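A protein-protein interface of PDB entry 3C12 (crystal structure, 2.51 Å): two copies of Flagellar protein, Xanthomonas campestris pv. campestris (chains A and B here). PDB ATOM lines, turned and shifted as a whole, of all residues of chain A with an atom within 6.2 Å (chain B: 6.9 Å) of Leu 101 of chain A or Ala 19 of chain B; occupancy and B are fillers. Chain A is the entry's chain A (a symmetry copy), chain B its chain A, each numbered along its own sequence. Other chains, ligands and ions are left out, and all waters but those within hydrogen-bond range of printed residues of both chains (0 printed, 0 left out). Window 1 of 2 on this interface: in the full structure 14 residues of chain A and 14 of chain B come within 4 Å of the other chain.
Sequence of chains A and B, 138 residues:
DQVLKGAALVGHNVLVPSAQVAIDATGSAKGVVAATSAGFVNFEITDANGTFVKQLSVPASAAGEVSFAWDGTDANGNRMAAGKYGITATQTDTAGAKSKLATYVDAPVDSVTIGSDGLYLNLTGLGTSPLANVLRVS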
ATOM      1  N   VAL A  33      -2.345  -7.036 -19.127  1.00  0.00           N
ATOM      2  CA  VAL A  33      -2.860  -8.089 -18.270  1.00  0.00           C
ATOM      3  C   VAL A  33      -4.289  -7.729 -17.892  1.00  0.00           C
ATOM      4  O   VAL A  33      -4.639  -6.552 -17.813  1.00  0.00           O
ATOM      5  CB  VAL A  33      -2.022  -8.220 -16.992  1.00  0.00           C
ATOM      6  CG1 VAL A  33      -2.719  -9.122 -16.016  1.00  0.00           C
ATOM      7  CG2 VAL A  33      -0.655  -8.780 -17.326  1.00  0.00           C
ATOM      8  N   ALA A  34      -5.117  -8.738 -17.657  1.00  0.00           N
ATOM      9  CA  ALA A  34      -6.499  -8.481 -17.301  1.00  0.00           C
ATOM     10  C   ALA A  34      -6.728  -8.561 -15.799  1.00  0.00           C
ATOM     11  O   ALA A  34      -6.812  -9.649 -15.237  1.00  0.00           O
ATOM     12  CB  ALA A  34      -7.399  -9.456 -18.025  1.00  0.00           C
ATOM     13  N   ALA A  35      -6.827  -7.393 -15.165  1.00  0.00           N
ATOM     14  CA  ALA A  35      -7.069  -7.280 -13.725  1.00  0.00           C
ATOM     15  C   ALA A  35      -8.509  -7.656 -13.419  1.00  0.00           C
ATOM     16  O   ALA A  35      -9.432  -7.207 -14.089  1.00  0.00           O
ATOM     17  CB  ALA A  35      -6.800  -5.863 -13.255  1.00  0.00           C
ATOM     18  N   THR A  36      -8.691  -8.473 -12.392  1.00  0.00           N
ATOM     19  CA  THR A  36     -10.014  -8.934 -12.013  1.00  0.00           C
ATOM     20  C   THR A  36     -10.634  -8.120 -10.884  1.00  0.00           C
ATOM     21  O   THR A  36     -11.756  -8.387 -10.454  1.00  0.00           O
ATOM     22  CB  THR A  36      -9.958 -10.398 -11.580  1.00  0.00           C
ATOM     23  OG1 THR A  36      -8.998 -10.542 -10.527  1.00  0.00           O
ATOM     24  CG2 THR A  36      -9.551 -11.277 -12.746  1.00  0.00           C
ATOM     25  N   VAL A  41      -1.173  -3.987  -9.737  1.00  0.00           N
ATOM     26  CA  VAL A  41      -0.559  -5.194 -10.237  1.00  0.00           C
ATOM     27  C   VAL A  41       0.939  -4.971 -10.309  1.00  0.00           C
ATOM     28  O   VAL A  41       1.401  -3.935 -10.777  1.00  0.00           O
ATOM     29  CB  VAL A  41      -1.114  -5.564 -11.622  1.00  0.00           C
ATOM     30  CG1 VAL A  41      -1.135  -4.346 -12.502  1.00  0.00           C
ATOM     31  CG2 VAL A  41      -0.274  -6.651 -12.248  1.00  0.00           C
ATOM     32  N   THR A  88       6.432 -11.979 -14.686  1.00  0.00           N
ATOM     33  CA  THR A  88       5.361 -12.493 -13.851  1.00  0.00           C
ATOM     34  C   THR A  88       4.514 -11.333 -13.342  1.00  0.00           C
ATOM     35  O   THR A  88       5.034 -10.287 -12.954  1.00  0.00           O
ATOM     36  CB  THR A  88       5.935 -13.282 -12.667  1.00  0.00           C
ATOM     37  OG1 THR A  88       6.622 -14.432 -13.169  1.00  0.00           O
ATOM     38  CG2 THR A  88       4.827 -13.729 -11.729  1.00  0.00           C
ATOM     39  N   ALA A  89       3.202 -11.517 -13.359  1.00  0.00           N
ATOM     40  CA  ALA A  89       2.310 -10.466 -12.910  1.00  0.00           C
ATOM     41  C   ALA A  89       1.470 -10.931 -11.754  1.00  0.00           C
ATOM     42  O   ALA A  89       0.832 -11.982 -11.808  1.00  0.00           O
ATOM     43  CB  ALA A  89       1.417 -10.018 -14.042  1.00  0.00           C
ATOM     44  N   THR A  90       1.482 -10.135 -10.694  1.00  0.00           N
ATOM     45  CA  THR A  90       0.704 -10.452  -9.513  1.00  0.00           C
ATOM     46  C   THR A  90      -0.191  -9.299  -9.147  1.00  0.00           C
ATOM     47  O   THR A  90       0.251  -8.158  -9.002  1.00  0.00           O
ATOM     48  CB  THR A  90       1.586 -10.752  -8.325  1.00  0.00           C
ATOM     49  OG1 THR A  90       2.586 -11.701  -8.707  1.00  0.00           O
ATOM     50  CG2 THR A  90       0.735 -11.317  -7.180  1.00  0.00           C
ATOM     51  N   GLN A  91      -1.462  -9.622  -8.989  1.00  0.00           N
ATOM     52  CA  GLN A  91      -2.464  -8.641  -8.640  1.00  0.00           C
ATOM     53  C   GLN A  91      -2.676  -8.652  -7.140  1.00  0.00           C
ATOM     54  O   GLN A  91      -2.552  -9.682  -6.478  1.00  0.00           O
ATOM     55  CB  GLN A  91      -3.781  -8.976  -9.341  1.00  0.00           C
ATOM     56  CG  GLN A  91      -4.856  -7.923  -9.216  1.00  0.00           C
ATOM     57  CD  GLN A  91      -6.242  -8.491  -9.426  1.00  0.00           C
ATOM     58  OE1 GLN A  91      -6.777  -9.161  -8.547  1.00  0.00           O
ATOM     59  NE2 GLN A  91      -6.828  -8.235 -10.596  1.00  0.00           N
ATOM     60  N   SER A  99      -3.095 -12.535  -6.368  1.00  0.00           N
ATOM     61  CA  SER A  99      -3.369 -13.493  -7.434  1.00  0.00           C
ATOM     62  C   SER A  99      -2.448 -13.290  -8.647  1.00  0.00           C
ATOM     63  O   SER A  99      -2.013 -12.172  -8.940  1.00  0.00           O
ATOM     64  CB  SER A  99      -4.845 -13.431  -7.863  1.00  0.00           C
ATOM     65  OG  SER A  99      -5.180 -12.188  -8.442  1.00  0.00           O
ATOM     66  N   LYS A 100      -2.130 -14.386  -9.329  1.00  0.00           N
ATOM     67  CA  LYS A 100      -1.279 -14.333 -10.513  1.00  0.00           C
ATOM     68  C   LYS A 100      -2.162 -14.137 -11.733  1.00  0.00           C
ATOM     69  O   LYS A 100      -3.172 -14.814 -11.893  1.00  0.00           O
ATOM     70  CB  LYS A 100      -0.463 -15.627 -10.653  1.00  0.00           C
ATOM     71  CG  LYS A 100       1.041 -15.441 -10.430  1.00  0.00           C
ATOM     72  CD  LYS A 100       1.831 -16.769 -10.427  1.00  0.00           C
ATOM     73  CE  LYS A 100       1.968 -17.437 -11.824  1.00  0.00           C
ATOM     74  NZ  LYS A 100       2.898 -16.767 -12.814  1.00  0.00           N
ATOM     75  N   LEU A 101      -1.788 -13.192 -12.583  1.00  0.00           N
ATOM     76  CA  LEU A 101      -2.557 -12.911 -13.789  1.00  0.00           C
ATOM     77  C   LEU A 101      -1.761 -13.304 -15.027  1.00  0.00           C
ATOM     78  O   LEU A 101      -0.534 -13.242 -15.020  1.00  0.00           O
ATOM     79  CB  LEU A 101      -2.897 -11.426 -13.865  1.00  0.00           C
ATOM     80  CG  LEU A 101      -3.562 -10.743 -12.668  1.00  0.00           C
ATOM     81  CD1 LEU A 101      -3.573  -9.254 -12.925  1.00  0.00           C
ATOM     82  CD2 LEU A 101      -4.975 -11.270 -12.439  1.00  0.00           C
ATOM     83  N   ALA A 102      -2.466 -13.704 -16.085  1.00  0.00           N
ATOM     84  CA  ALA A 102      -1.833 -14.102 -17.342  1.00  0.00           C
ATOM     85  C   ALA A 102      -1.290 -12.884 -18.061  1.00  0.00           C
ATOM     86  O   ALA A 102      -1.965 -11.870 -18.170  1.00  0.00           O
ATOM     87  CB  ALA A 102      -2.831 -14.810 -18.228  1.00  0.00           C
ATOM     88  N   THR A 103      -0.068 -12.988 -18.560  1.00  0.00           N
ATOM     89  CA  THR A 103       0.552 -11.878 -19.265  1.00  0.00           C
ATOM     90  C   THR A 103       0.450 -12.011 -20.779  1.00  0.00           C
ATOM     91  O   THR A 103       0.652 -13.090 -21.332  1.00  0.00           O
ATOM     92  CB  THR A 103       2.040 -11.751 -18.885  1.00  0.00           C
ATOM     93  OG1 THR A 103       2.604 -13.057 -18.722  1.00  0.00           O
ATOM     94  CG2 THR A 103       2.199 -10.981 -17.596  1.00  0.00           C
ATOM     95  N   VAL B  16      -7.204 -22.227 -22.255  1.00  0.00           N
ATOM     96  CA  VAL B  16      -7.020 -20.792 -22.229  1.00  0.00           C
ATOM     97  C   VAL B  16      -5.752 -20.445 -21.469  1.00  0.00           C
ATOM     98  O   VAL B  16      -5.337 -21.166 -20.564  1.00  0.00           O
ATOM     99  CB  VAL B  16      -8.216 -20.097 -21.548  1.00  0.00           C
ATOM    100  CG1 VAL B  16      -9.469 -20.303 -22.370  1.00  0.00           C
ATOM    101  CG2 VAL B  16      -8.413 -20.659 -20.153  1.00  0.00           C
ATOM    102  N   PRO B  17      -5.104 -19.343 -21.853  1.00  0.00           N
ATOM    103  CA  PRO B  17      -3.876 -18.893 -21.199  1.00  0.00           C
ATOM    104  C   PRO B  17      -4.214 -18.494 -19.770  1.00  0.00           C
ATOM    105  O   PRO B  17      -5.033 -17.606 -19.554  1.00  0.00           O
ATOM    106  CB  PRO B  17      -3.459 -17.691 -22.040  1.00  0.00           C
ATOM    107  CG  PRO B  17      -4.003 -18.016 -23.383  1.00  0.00           C
ATOM    108  CD  PRO B  17      -5.368 -18.550 -23.062  1.00  0.00           C
ATOM    109  N   SER B  18      -3.592 -19.148 -18.796  1.00  0.00           N
ATOM    110  CA  SER B  18      -3.864 -18.834 -17.400  1.00  0.00           C
ATOM    111  C   SER B  18      -2.604 -18.936 -16.561  1.00  0.00           C
ATOM    112  O   SER B  18      -1.812 -19.852 -16.738  1.00  0.00           O
ATOM    113  CB  SER B  18      -4.936 -19.784 -16.852  1.00  0.00           C
ATOM    114  OG  SER B  18      -5.314 -19.433 -15.539  1.00  0.00           O
ATOM    115  N   ALA B  19      -2.416 -17.982 -15.659  1.00  0.00           N
ATOM    116  CA  ALA B  19      -1.252 -17.983 -14.787  1.00  0.00           C
ATOM    117  C   ALA B  19      -1.558 -18.819 -13.557  1.00  0.00           C
ATOM    118  O   ALA B  19      -0.684 -19.066 -12.736  1.00  0.00           O
ATOM    119  CB  ALA B  19      -0.899 -16.567 -14.377  1.00  0.00           C
ATOM    120  N   GLN B  20      -2.805 -19.252 -13.427  1.00  0.00           N
ATOM    121  CA  GLN B  20      -3.196 -20.070 -12.292  1.00  0.00           C
ATOM    122  C   GLN B  20      -4.104 -21.217 -12.701  1.00  0.00           C
ATOM    123  O   GLN B  20      -4.662 -21.225 -13.791  1.00  0.00           O
ATOM    124  CB  GLN B  20      -3.860 -19.207 -11.203  1.00  0.00           C
ATOM    125  CG  GLN B  20      -4.918 -18.220 -11.677  1.00  0.00           C
ATOM    126  CD  GLN B  20      -5.420 -17.305 -10.562  1.00  0.00           C
ATOM    127  OE1 GLN B  20      -4.632 -16.672  -9.864  1.00  0.00           O
ATOM    128  NE2 GLN B  20      -6.735 -17.228 -10.403  1.00  0.00           N
ATOM    129  N   VAL B  21      -4.215 -22.205 -11.823  1.00  0.00           N
ATOM    130  CA  VAL B  21      -5.056 -23.372 -12.059  1.00  0.00           C
ATOM    131  C   VAL B  21      -5.996 -23.490 -10.869  1.00  0.00           C
ATOM    132  O   VAL B  21      -5.764 -22.881  -9.834  1.00  0.00           O
ATOM    133  CB  VAL B  21      -4.215 -24.660 -12.161  1.00  0.00           C
ATOM    134  CG1 VAL B  21      -3.204 -24.534 -13.283  1.00  0.00           C
ATOM    135  CG2 VAL B  21      -3.507 -24.919 -10.855  1.00  0.00           C
ATOM    136  N   THR B  46       2.273 -22.497  -6.692  1.00  0.00           N
ATOM    137  CA  THR B  46       2.383 -21.671  -5.494  1.00  0.00           C
ATOM    138  C   THR B  46       0.993 -21.286  -4.988  1.00  0.00           C
ATOM    139  O   THR B  46       0.004 -21.423  -5.711  1.00  0.00           O
ATOM    140  CB  THR B  46       3.202 -20.402  -5.760  1.00  0.00           C
ATOM    141  OG1 THR B  46       2.623 -19.678  -6.848  1.00  0.00           O
ATOM    142  CG2 THR B  46       4.631 -20.761  -6.101  1.00  0.00           C
ATOM    143  N   TYR B  85      -4.767 -21.670  -7.673  1.00  0.00           N
ATOM    144  CA  TYR B  85      -3.354 -21.683  -7.341  1.00  0.00           C
ATOM    145  C   TYR B  85      -2.548 -21.180  -8.517  1.00  0.00           C
ATOM    146  O   TYR B  85      -2.928 -21.393  -9.671  1.00  0.00           O
ATOM    147  CB  TYR B  85      -2.895 -23.094  -6.986  1.00  0.00           C
ATOM    148  CG  TYR B  85      -3.437 -23.587  -5.683  1.00  0.00           C
ATOM    149  CD1 TYR B  85      -4.737 -24.082  -5.581  1.00  0.00           C
ATOM    150  CD2 TYR B  85      -2.660 -23.527  -4.533  1.00  0.00           C
ATOM    151  CE1 TYR B  85      -5.248 -24.503  -4.363  1.00  0.00           C
ATOM    152  CE2 TYR B  85      -3.157 -23.947  -3.306  1.00  0.00           C
ATOM    153  CZ  TYR B  85      -4.447 -24.431  -3.229  1.00  0.00           C
ATOM    154  OH  TYR B  85      -4.921 -24.835  -2.004  1.00  0.00           O
ATOM    155  N   GLY B  86      -1.432 -20.517  -8.221  1.00  0.00           N
ATOM    156  CA  GLY B  86      -0.584 -20.002  -9.279  1.00  0.00           C
ATOM    157  C   GLY B  86       0.331 -21.065  -9.858  1.00  0.00           C
ATOM    158  O   GLY B  86       0.843 -21.918  -9.134  1.00  0.00           O
ATOM    159  N   ILE B  87       0.527 -21.030 -11.169  1.00  0.00           N
ATOM    160  CA  ILE B  87       1.403 -21.998 -11.810  1.00  0.00           C
ATOM    161  C   ILE B  87       2.419 -21.342 -12.737  1.00  0.00           C
ATOM    162  O   ILE B  87       2.085 -20.496 -13.566  1.00  0.00           O
ATOM    163  CB  ILE B  87       0.614 -23.065 -12.613  1.00  0.00           C
ATOM    164  CG1 ILE B  87       1.610 -24.020 -13.273  1.00  0.00           C
ATOM    165  CG2 ILE B  87      -0.281 -22.413 -13.653  1.00  0.00           C
ATOM    166  CD1 ILE B  87       0.989 -25.022 -14.189  1.00  0.00           C
ATOM    167  N   THR B  88       3.671 -21.745 -12.577  1.00  0.00           N
ATOM    168  CA  THR B  88       4.763 -21.230 -13.384  1.00  0.00           C
ATOM    169  C   THR B  88       5.483 -22.390 -14.060  1.00  0.00           C
ATOM    170  O   THR B  88       5.719 -23.435 -13.453  1.00  0.00           O
ATOM    171  CB  THR B  88       5.747 -20.439 -12.514  1.00  0.00           C
ATOM    172  OG1 THR B  88       5.077 -19.288 -11.990  1.00  0.00           O
ATOM    173  CG2 THR B  88       6.949 -19.991 -13.328  1.00  0.00           C
ATOM    174  N   THR B 103       1.693 -20.753 -19.883  1.00  0.00           N
ATOM    175  CA  THR B 103       0.848 -21.864 -19.474  1.00  0.00           C
ATOM    176  C   THR B 103      -0.582 -21.734 -19.981  1.00  0.00           C
ATOM    177  O   THR B 103      -1.171 -20.655 -19.938  1.00  0.00           O
ATOM    178  CB  THR B 103       0.813 -21.988 -17.939  1.00  0.00           C
ATOM    179  OG1 THR B 103       0.816 -20.680 -17.355  1.00  0.00           O
ATOM    180  CG2 THR B 103       2.013 -22.755 -17.437  1.00  0.00           C
ATOM    181  N   VAL B 105      -4.268 -23.457 -19.459  1.00  0.00           N
ATOM    182  CA  VAL B 105      -5.026 -24.336 -18.593  1.00  0.00           C
ATOM    183  C   VAL B 105      -6.274 -24.888 -19.232  1.00  0.00           C
ATOM    184  O   VAL B 105      -6.975 -24.185 -19.968  1.00  0.00           O
ATOM    185  CB  VAL B 105      -5.434 -23.605 -17.316  1.00  0.00           C
ATOM    186  CG1 VAL B 105      -6.220 -24.526 -16.419  1.00  0.00           C
ATOM    187  CG2 VAL B 105      -4.205 -23.087 -16.622  1.00  0.00           C
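Of chain B, only Ala 19 (3.4 Å) comes within 4 Å of Leu 101 of chain A.
Printed residues of chain A within 4 Å of Pro 17 of chain B: Ala 102.
Of the printed residues of chain A, Ala 19 of chain B touches Lys 100 (3.2 Å), Leu 101 (3.4 Å) and Ala 102 (3.7 Å).
Of the printed residues of chain A, Gln 20 of chain B touches Ser 99 and Lys 100.
Of the printed residues of chain A, Thr 88 of chain B touches Lys 100.
The side-chain hydroxyl (OG1) of Thr 88 of chain B is in hydrogen-bond range of the side-chain amino group (NZ) of Lys 100 of chain A, 3.4 Å away.
The side-chain amide oxygen of Gln 20 of chain B lies close to the backbone carbonyl oxygen of Lys 100 of chain A (3.1 Å).
Gln 20 of chain B touches Ser 99 of chain A.
Ala 19 of chain B touches Lys 100 of chain A (O to CE, 3.2 Å).
O of Ile 87 of chain B touches CE of Lys 100 of chain A, 3.5 Å away.
Leu 101 of chain A touches Ala 19 of chain B.
Pro 17 of chain B touches Ala 102 of chain A (O to CB, 3.8 Å).
Ala 102 of chain A touches Ala 19 of chain B (N to CB, 3.7 Å).
Of the 14 printed residues of chain A, 4 touch a printed residue of chain B.
Hydrophobic or aromatic side chains of chain B within 4 Å of the printed part of chain A: Ala 19.
Among the printed residues, 8 pairs touch across the chains.
Among the printed residues, no Asp or Glu carboxylate lies within 4 Å of a Lys or Arg side-chain nitrogen of the other chain.
2 positions are printed for both chains.
N of Ile 87 of chain B lies within hydrogen-bond range of O of Ala 19 of chain B (2.8 Å).
OG of Ser 18 of chain B sits at hydrogen-bond distance from O of Gln 20 of chain B, 2.6 Å away.
The backbone NH of Gln 91 of chain A lies within hydrogen-bond range of the backbone carbonyl oxygen of Ser 99 of chain A.
O of Ala 89 of chain A sits at hydrogen-bond distance from N of Leu 101 of chain A, at 3.0 Å.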
